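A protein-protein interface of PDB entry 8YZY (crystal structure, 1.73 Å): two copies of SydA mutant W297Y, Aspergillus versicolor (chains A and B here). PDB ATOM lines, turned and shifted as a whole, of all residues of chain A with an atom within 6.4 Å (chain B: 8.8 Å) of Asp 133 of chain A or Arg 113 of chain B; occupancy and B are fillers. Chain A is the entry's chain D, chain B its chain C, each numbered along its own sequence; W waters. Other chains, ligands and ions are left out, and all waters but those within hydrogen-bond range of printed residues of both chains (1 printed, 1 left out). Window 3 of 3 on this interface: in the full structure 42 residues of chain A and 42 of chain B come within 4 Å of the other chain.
NH2 of Arg 113 of chain B lies within salt-bridge range of OD2 of Asp 133 of chain A, at 2.8 Å.
The guanidinium group (NE) of Arg 113 of chain B sits at hydrogen-bond distance from the backbone carbonyl oxygen (O) of Gln 130 of chain A.
NE2 of Gln 130 of chain A lies within hydrogen-bond range of O of Val 112 of chain B (2.9 Å).
The backbone carbonyl oxygen (O) of Leu 129 of chain A lies within hydrogen-bond range of the side-chain hydroxyl (OG1) of Thr 132 of chain A, 3.3 Å away.
The side-chain hydroxyl (OG1) of Thr 132 of chain A is in hydrogen-bond range of the side-chain hydroxyl (OG) of Ser 141 of chain A (2.9 Å).
Leu 111 of chain A touches Leu 111 of chain B (O to O, 3.9 Å).
CG1 of Val 112 of chain B touches CD2 of Leu 111 of chain A, at 3.6 Å.
CD2 of Leu 109 of chain B touches O of Leu 129 of chain A, at 3.6 Å.
Leu 109 of chain B touches Thr 132 of chain A.
CD1 of Leu 109 of chain B touches CB of Asp 133 of chain A, 3.7 Å away.
Of the printed residues of chain B, Leu 111 of chain A touches Leu 111 (3.9 Å) and Val 112 (3.6 Å).
Of the printed residues of chain B, Leu 129 of chain A touches Leu 109.
Printed residues of chain B within 4 Å of Gln 130 of chain A: Val 112 (2.9 Å) and Arg 113 (3.0 Å).
Asn 131 of chain A touches none of the printed residues of chain B.
Printed residues of chain B within 4 Å of Asp 133 of chain A: Leu 109 (3.7 Å) and Arg 113 (2.8 Å).
Of the printed residues of chain A, Leu 109 of chain B touches Leu 129 (3.6 Å), Thr 132 (3.9 Å) and Asp 133 (3.7 Å).
Of the printed residues of chain A, Leu 111 of chain B touches Leu 111.
The nearest residue of chain A that does not touch Arg 113 of chain B is Asn 131 of chain A (4.6 Å).
Of the 13 printed residues of chain B, 4 touch a printed residue of chain A.
Printed residues of chain B that touch a printed residue of chain A: Leu 109, Leu 111, Val 112 and Arg 113.
Hydrophobic or aromatic side chains of chain B within 4 Å of the printed part of chain A: Leu 109 and Val 112.
Along chain B the printed residues that touch a printed residue of chain A span positions 109 to 113.
Along chain A the printed residues that touch a printed residue of chain B span positions 111 to 133.
Among the printed residues, Asp or Glu carboxylates within 4 Å of a Lys or Arg side-chain nitrogen of the other chain: Asp 133 of chain A with Arg 113 of chain B.
Leu 111 of chain A touches its own counterpart, Leu 111 of chain B.
3 positions are printed for both chains.
Of the 8 pairs that touch across the chains among the printed residues, 1 has its exchanged pair printed and touching as well.
Water W1 lies within hydrogen-bond range of O of Leu 111 of chain A (2.9 Å), O of Val 112 of chain B (3.1 Å) and NE2 of Gln 130 of chain A (3.2 Å).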
ATOM      1  N   LEU A 111      27.824  28.188  15.679  1.00  0.00           N
ATOM      2  CA  LEU A 111      26.836  27.329  15.042  1.00  0.00           C
ATOM      3  C   LEU A 111      27.477  26.552  13.902  1.00  0.00           C
ATOM      4  O   LEU A 111      27.381  25.319  13.855  1.00  0.00           O
ATOM      5  CB  LEU A 111      25.654  28.164  14.545  1.00  0.00           C
ATOM      6  CG  LEU A 111      24.542  27.377  13.831  1.00  0.00           C
ATOM      7  CD1 LEU A 111      23.741  26.587  14.897  1.00  0.00           C
ATOM      8  CD2 LEU A 111      23.634  28.340  13.017  1.00  0.00           C
ATOM      9  N   GLY A 114      29.898  23.835  14.911  1.00  0.00           N
ATOM     10  CA  GLY A 114      29.408  22.755  15.771  1.00  0.00           C
ATOM     11  C   GLY A 114      29.880  22.811  17.211  1.00  0.00           C
ATOM     12  O   GLY A 114      30.136  21.765  17.826  1.00  0.00           O
ATOM     13  N   PHE A 128      17.038  24.127  17.354  1.00  0.00           N
ATOM     14  CA  PHE A 128      15.890  24.436  16.511  1.00  0.00           C
ATOM     15  C   PHE A 128      16.306  24.515  15.047  1.00  0.00           C
ATOM     16  O   PHE A 128      15.649  23.923  14.162  1.00  0.00           O
ATOM     17  CB  PHE A 128      15.224  25.736  16.958  1.00  0.00           C
ATOM     18  CG  PHE A 128      13.974  26.059  16.169  1.00  0.00           C
ATOM     19  CD1 PHE A 128      14.064  26.738  14.973  1.00  0.00           C
ATOM     20  CD2 PHE A 128      12.733  25.584  16.588  1.00  0.00           C
ATOM     21  CE1 PHE A 128      12.933  26.998  14.214  1.00  0.00           C
ATOM     22  CE2 PHE A 128      11.583  25.860  15.849  1.00  0.00           C
ATOM     23  CZ  PHE A 128      11.688  26.546  14.648  1.00  0.00           C
ATOM     24  N   LEU A 129      17.375  25.284  14.771  1.00  0.00           N
ATOM     25  CA  LEU A 129      17.808  25.430  13.383  1.00  0.00           C
ATOM     26  C   LEU A 129      18.230  24.087  12.798  1.00  0.00           C
ATOM     27  O   LEU A 129      18.039  23.840  11.598  1.00  0.00           O
ATOM     28  CB  LEU A 129      18.951  26.432  13.283  1.00  0.00           C
ATOM     29  CG  LEU A 129      18.650  27.861  13.723  1.00  0.00           C
ATOM     30  CD1 LEU A 129      19.908  28.755  13.539  1.00  0.00           C
ATOM     31  CD2 LEU A 129      17.423  28.403  12.951  1.00  0.00           C
ATOM     32  N   GLN A 130      18.772  23.205  13.642  1.00  0.00           N
ATOM     33  CA  GLN A 130      19.218  21.888  13.184  1.00  0.00           C
ATOM     34  C   GLN A 130      18.059  20.974  12.830  1.00  0.00           C
ATOM     35  O   GLN A 130      18.269  19.931  12.194  1.00  0.00           O
ATOM     36  CB  GLN A 130      20.075  21.240  14.274  1.00  0.00           C
ATOM     37  CG  GLN A 130      21.458  21.861  14.378  1.00  0.00           C
ATOM     38  CD  GLN A 130      22.125  21.543  15.704  1.00  0.00           C
ATOM     39  OE1 GLN A 130      21.554  20.833  16.531  1.00  0.00           O
ATOM     40  NE2 GLN A 130      23.333  22.057  15.910  1.00  0.00           N
ATOM     41  N   ASN A 131      16.852  21.300  13.297  1.00  0.00           N
ATOM     42  CA  ASN A 131      15.719  20.402  13.069  1.00  0.00           C
ATOM     43  C   ASN A 131      14.557  21.038  12.309  1.00  0.00           C
ATOM     44  O   ASN A 131      13.452  20.478  12.317  1.00  0.00           O
ATOM     45  CB  ASN A 131      15.263  19.839  14.413  1.00  0.00           C
ATOM     46  CG  ASN A 131      16.294  18.868  14.977  1.00  0.00           C
ATOM     47  OD1 ASN A 131      16.405  17.733  14.501  1.00  0.00           O
ATOM     48  ND2 ASN A 131      17.141  19.357  15.881  1.00  0.00           N
ATOM     49  N   THR A 132      14.783  22.185  11.650  1.00  0.00           N
ATOM     50  CA  THR A 132      13.749  22.747  10.759  1.00  0.00           C
ATOM     51  C   THR A 132      13.249  21.773   9.681  1.00  0.00           C
ATOM     52  O   THR A 132      12.141  21.971   9.162  1.00  0.00           O
ATOM     53  CB  THR A 132      14.230  24.042  10.062  1.00  0.00           C
ATOM     54  OG1 THR A 132      15.504  23.841   9.445  1.00  0.00           O
ATOM     55  CG2 THR A 132      14.349  25.202  11.071  1.00  0.00           C
ATOM     56  N   ASP A 133      14.013  20.726   9.323  1.00  0.00           N
ATOM     57  CA  ASP A 133      13.486  19.781   8.344  1.00  0.00           C
ATOM     58  C   ASP A 133      12.283  19.004   8.870  1.00  0.00           C
ATOM     59  O   ASP A 133      11.640  18.292   8.085  1.00  0.00           O
ATOM     60  CB  ASP A 133      14.566  18.798   7.860  1.00  0.00           C
ATOM     61  CG  ASP A 133      15.266  18.049   8.991  1.00  0.00           C
ATOM     62  OD1 ASP A 133      15.171  18.454  10.175  1.00  0.00           O
ATOM     63  OD2 ASP A 133      15.938  17.038   8.671  1.00  0.00           O
ATOM     64  N   GLN A 134      11.975  19.114  10.169  1.00  0.00           N
ATOM     65  CA  GLN A 134      10.730  18.564  10.699  1.00  0.00           C
ATOM     66  C   GLN A 134       9.493  19.218  10.079  1.00  0.00           C
ATOM     67  O   GLN A 134       8.422  18.603  10.059  1.00  0.00           O
ATOM     68  CB  GLN A 134      10.675  18.747  12.215  1.00  0.00           C
ATOM     69  CG  GLN A 134      11.637  17.868  12.999  1.00  0.00           C
ATOM     70  CD  GLN A 134      11.405  16.394  12.762  1.00  0.00           C
ATOM     71  OE1 GLN A 134      12.285  15.695  12.262  1.00  0.00           O
ATOM     72  NE2 GLN A 134      10.213  15.912  13.109  1.00  0.00           N
ATOM     73  N   TYR A 135       9.587  20.477   9.631  1.00  0.00           N
ATOM     74  CA  TYR A 135       8.397  21.099   9.065  1.00  0.00           C
ATOM     75  C   TYR A 135       8.626  21.884   7.774  1.00  0.00           C
ATOM     76  O   TYR A 135       7.635  22.249   7.134  1.00  0.00           O
ATOM     77  CB  TYR A 135       7.718  22.005  10.115  1.00  0.00           C
ATOM     78  CG  TYR A 135       8.426  23.307  10.448  1.00  0.00           C
ATOM     79  CD1 TYR A 135       9.620  23.321  11.182  1.00  0.00           C
ATOM     80  CD2 TYR A 135       7.878  24.526  10.065  1.00  0.00           C
ATOM     81  CE1 TYR A 135      10.260  24.520  11.475  1.00  0.00           C
ATOM     82  CE2 TYR A 135       8.505  25.719  10.363  1.00  0.00           C
ATOM     83  CZ  TYR A 135       9.685  25.708  11.075  1.00  0.00           C
ATOM     84  OH  TYR A 135      10.299  26.902  11.357  1.00  0.00           O
ATOM     85  N   LEU A 136       9.872  22.123   7.342  1.00  0.00           N
ATOM     86  CA  LEU A 136      10.164  22.810   6.085  1.00  0.00           C
ATOM     87  C   LEU A 136      11.000  21.939   5.165  1.00  0.00           C
ATOM     88  O   LEU A 136      11.737  21.053   5.617  1.00  0.00           O
ATOM     89  CB  LEU A 136      10.928  24.112   6.335  1.00  0.00           C
ATOM     90  CG  LEU A 136      10.151  25.062   7.251  1.00  0.00           C
ATOM     91  CD1 LEU A 136      11.011  26.248   7.561  1.00  0.00           C
ATOM     92  CD2 LEU A 136       8.844  25.469   6.579  1.00  0.00           C
ATOM     93  N   GLY A 137      10.891  22.222   3.860  1.00  0.00           N
ATOM     94  CA  GLY A 137      11.808  21.654   2.897  1.00  0.00           C
ATOM     95  C   GLY A 137      13.160  22.342   2.972  1.00  0.00           C
ATOM     96  O   GLY A 137      13.402  23.208   3.798  1.00  0.00           O
ATOM     97  N   SER A 141      14.305  25.599   5.100  1.00  0.00           N
ATOM     98  CA  SER A 141      15.248  25.425   6.210  1.00  0.00           C
ATOM     99  C   SER A 141      16.407  26.395   6.084  1.00  0.00           C
ATOM    100  O   SER A 141      16.842  27.007   7.075  1.00  0.00           O
ATOM    101  CB  SER A 141      15.840  23.995   6.235  1.00  0.00           C
ATOM    102  OG  SER A 141      14.968  23.014   6.750  1.00  0.00           O
ATOM    103  N   ASN A 193       5.964  22.319   4.216  1.00  0.00           N
ATOM    104  CA  ASN A 193       6.450  21.247   3.346  1.00  0.00           C
ATOM    105  C   ASN A 193       5.510  20.041   3.283  1.00  0.00           C
ATOM    106  O   ASN A 193       5.541  19.297   2.297  1.00  0.00           O
ATOM    107  CB  ASN A 193       7.832  20.801   3.831  1.00  0.00           C
ATOM    108  CG  ASN A 193       8.596  20.049   2.788  1.00  0.00           C
ATOM    109  OD1 ASN A 193       8.709  20.491   1.634  1.00  0.00           O
ATOM    110  ND2 ASN A 193       9.169  18.912   3.189  1.00  0.00           N
ATOM    111  N   GLU B 106      21.828  19.677   0.730  1.00  0.00           N
ATOM    112  CA  GLU B 106      22.038  19.348   2.149  1.00  0.00           C
ATOM    113  C   GLU B 106      22.966  20.317   2.860  1.00  0.00           C
ATOM    114  O   GLU B 106      23.131  20.216   4.095  1.00  0.00           O
ATOM    115  CB  GLU B 106      22.593  17.912   2.291  1.00  0.00           C
ATOM    116  CG  GLU B 106      21.799  16.861   1.514  1.00  0.00           C
ATOM    117  CD  GLU B 106      21.865  15.477   2.139  1.00  0.00           C
ATOM    118  OE1 GLU B 106      22.483  15.329   3.219  1.00  0.00           O
ATOM    119  OE2 GLU B 106      21.314  14.531   1.532  1.00  0.00           O
ATOM    120  N   PHE B 107      23.540  21.274   2.123  1.00  0.00           N
ATOM    121  CA  PHE B 107      24.629  22.077   2.672  1.00  0.00           C
ATOM    122  C   PHE B 107      24.237  22.750   3.981  1.00  0.00           C
ATOM    123  O   PHE B 107      24.897  22.540   5.019  1.00  0.00           O
ATOM    124  CB  PHE B 107      25.069  23.127   1.637  1.00  0.00           C
ATOM    125  CG  PHE B 107      26.209  23.973   2.113  1.00  0.00           C
ATOM    126  CD1 PHE B 107      27.502  23.451   2.143  1.00  0.00           C
ATOM    127  CD2 PHE B 107      26.004  25.302   2.483  1.00  0.00           C
ATOM    128  CE1 PHE B 107      28.575  24.212   2.570  1.00  0.00           C
ATOM    129  CE2 PHE B 107      27.084  26.076   2.913  1.00  0.00           C
ATOM    130  CZ  PHE B 107      28.373  25.516   2.977  1.00  0.00           C
ATOM    131  N   SER B 108      23.098  23.476   3.980  1.00  0.00           N
ATOM    132  CA  SER B 108      22.789  24.303   5.144  1.00  0.00           C
ATOM    133  C   SER B 108      22.526  23.447   6.373  1.00  0.00           C
ATOM    134  O   SER B 108      23.050  23.752   7.450  1.00  0.00           O
ATOM    135  CB  SER B 108      21.611  25.259   4.900  1.00  0.00           C
ATOM    136  OG  SER B 108      20.413  24.568   4.597  1.00  0.00           O
ATOM    137  N   LEU B 109      21.788  22.339   6.226  1.00  0.00           N
ATOM    138  CA  LEU B 109      21.506  21.547   7.426  1.00  0.00           C
ATOM    139  C   LEU B 109      22.771  20.845   7.913  1.00  0.00           C
ATOM    140  O   LEU B 109      23.055  20.824   9.129  1.00  0.00           O
ATOM    141  CB  LEU B 109      20.364  20.558   7.154  1.00  0.00           C
ATOM    142  CG  LEU B 109      18.974  21.198   7.294  1.00  0.00           C
ATOM    143  CD1 LEU B 109      17.861  20.192   7.072  1.00  0.00           C
ATOM    144  CD2 LEU B 109      18.813  21.883   8.666  1.00  0.00           C
ATOM    145  N   ARG B 110      23.601  20.345   6.983  1.00  0.00           N
ATOM    146  CA  ARG B 110      24.828  19.717   7.472  1.00  0.00           C
ATOM    147  C   ARG B 110      25.715  20.744   8.122  1.00  0.00           C
ATOM    148  O   ARG B 110      26.350  20.459   9.148  1.00  0.00           O
ATOM    149  CB  ARG B 110      25.563  18.999   6.343  1.00  0.00           C
ATOM    150  CG  ARG B 110      24.860  17.716   6.001  1.00  0.00           C
ATOM    151  CD  ARG B 110      25.571  17.009   4.905  1.00  0.00           C
ATOM    152  NE  ARG B 110      24.948  15.726   4.612  1.00  0.00           N
ATOM    153  CZ  ARG B 110      25.600  14.580   4.526  1.00  0.00           C
ATOM    154  NH1 ARG B 110      26.894  14.507   4.783  1.00  0.00           N
ATOM    155  NH2 ARG B 110      24.959  13.508   4.076  1.00  0.00           N
ATOM    156  N   LEU B 111      25.698  21.971   7.592  1.00  0.00           N
ATOM    157  CA  LEU B 111      26.533  23.013   8.144  1.00  0.00           C
ATOM    158  C   LEU B 111      26.147  23.295   9.586  1.00  0.00           C
ATOM    159  O   LEU B 111      27.016  23.356  10.469  1.00  0.00           O
ATOM    160  CB  LEU B 111      26.400  24.288   7.308  1.00  0.00           C
ATOM    161  CG  LEU B 111      27.364  25.403   7.681  1.00  0.00           C
ATOM    162  CD1 LEU B 111      28.805  25.004   7.378  1.00  0.00           C
ATOM    163  CD2 LEU B 111      26.946  26.695   6.965  1.00  0.00           C
ATOM    164  N   VAL B 112      24.839  23.448   9.853  1.00  0.00           N
ATOM    165  CA  VAL B 112      24.504  23.893  11.210  1.00  0.00           C
ATOM    166  C   VAL B 112      24.458  22.740  12.202  1.00  0.00           C
ATOM    167  O   VAL B 112      24.433  22.985  13.413  1.00  0.00           O
ATOM    168  CB  VAL B 112      23.187  24.683  11.307  1.00  0.00           C
ATOM    169  CG1 VAL B 112      23.275  25.922  10.427  1.00  0.00           C
ATOM    170  CG2 VAL B 112      21.987  23.810  10.905  1.00  0.00           C
ATOM    171  N   ARG B 113      24.451  21.497  11.721  1.00  0.00           N
ATOM    172  CA  ARG B 113      24.584  20.314  12.561  1.00  0.00           C
ATOM    173  C   ARG B 113      26.032  19.998  12.881  1.00  0.00           C
ATOM    174  O   ARG B 113      26.280  19.073  13.660  1.00  0.00           O
ATOM    175  CB  ARG B 113      23.958  19.083  11.874  1.00  0.00           C
ATOM    176  CG  ARG B 113      22.425  19.172  11.780  1.00  0.00           C
ATOM    177  CD  ARG B 113      21.799  18.067  10.941  1.00  0.00           C
ATOM    178  NE  ARG B 113      20.342  18.183  10.929  1.00  0.00           N
ATOM    179  CZ  ARG B 113      19.541  17.468  10.152  1.00  0.00           C
ATOM    180  NH1 ARG B 113      20.024  16.599   9.279  1.00  0.00           N
ATOM    181  NH2 ARG B 113      18.224  17.620  10.262  1.00  0.00           N
ATOM    182  N   GLY B 114      26.980  20.723  12.289  1.00  0.00           N
ATOM    183  CA  GLY B 114      28.389  20.442  12.485  1.00  0.00           C
ATOM    184  C   GLY B 114      28.814  19.151  11.837  1.00  0.00           C
ATOM    185  O   GLY B 114      29.752  18.501  12.322  1.00  0.00           O
ATOM    186  N   LEU B 115      28.104  18.722  10.720  1.00  0.00           N
ATOM    187  CA  LEU B 115      28.398  17.464  10.017  1.00  0.00           C
ATOM    188  C   LEU B 115      29.280  17.732   8.807  1.00  0.00           C
ATOM    189  O   LEU B 115      29.255  18.821   8.224  1.00  0.00           O
ATOM    190  CB  LEU B 115      27.100  16.816   9.523  1.00  0.00           C
ATOM    191  CG  LEU B 115      26.117  16.399  10.609  1.00  0.00           C
ATOM    192  CD1 LEU B 115      24.849  15.886   9.993  1.00  0.00           C
ATOM    193  CD2 LEU B 115      26.757  15.332  11.464  1.00  0.00           C
ATOM    194  N   PRO B 116      30.061  16.745   8.403  1.00  0.00           N
ATOM    195  CA  PRO B 116      30.758  16.845   7.121  1.00  0.00           C
ATOM    196  C   PRO B 116      29.762  16.939   5.975  1.00  0.00           C
ATOM    197  O   PRO B 116      28.632  16.449   6.056  1.00  0.00           O
ATOM    198  CB  PRO B 116      31.567  15.546   7.045  1.00  0.00           C
ATOM    199  CG  PRO B 116      30.839  14.584   7.928  1.00  0.00           C
ATOM    200  CD  PRO B 116      30.157  15.423   9.025  1.00  0.00           C
ATOM    201  N   GLN B 117      30.208  17.567   4.897  1.00  0.00           N
ATOM    202  CA  GLN B 117      29.370  17.715   3.715  1.00  0.00           C
ATOM    203  C   GLN B 117      29.402  16.451   2.844  1.00  0.00           C
ATOM    204  O   GLN B 117      30.215  15.540   3.031  1.00  0.00           O
ATOM    205  CB  GLN B 117      29.812  18.950   2.928  1.00  0.00           C
ATOM    206  CG  GLN B 117      29.678  20.246   3.705  1.00  0.00           C
ATOM    207  CD  GLN B 117      28.224  20.624   3.945  1.00  0.00           C
ATOM    208  OE1 GLN B 117      27.330  20.228   3.191  1.00  0.00           O
ATOM    209  NE2 GLN B 117      27.987  21.411   4.986  1.00  0.00           N
ATOM    210  N   GLN B 130      33.592  28.763   8.458  1.00  0.00           N
ATOM    211  CA  GLN B 130      33.979  28.627   9.856  1.00  0.00           C
ATOM    212  C   GLN B 130      35.122  29.552  10.217  1.00  0.00           C
ATOM    213  O   GLN B 130      35.362  29.803  11.410  1.00  0.00           O
ATOM    214  CB  GLN B 130      34.402  27.187  10.174  1.00  0.00           C
ATOM    215  CG  GLN B 130      33.245  26.190  10.248  1.00  0.00           C
ATOM    216  CD  GLN B 130      33.727  24.738  10.113  1.00  0.00           C
ATOM    217  OE1 GLN B 130      34.909  24.493   9.908  1.00  0.00           O
ATOM    218  NE2 GLN B 130      32.820  23.783  10.284  1.00  0.00           N
HETATM  219  O   HOH W   1      26.027  23.839  15.906  1.00  0.00           O
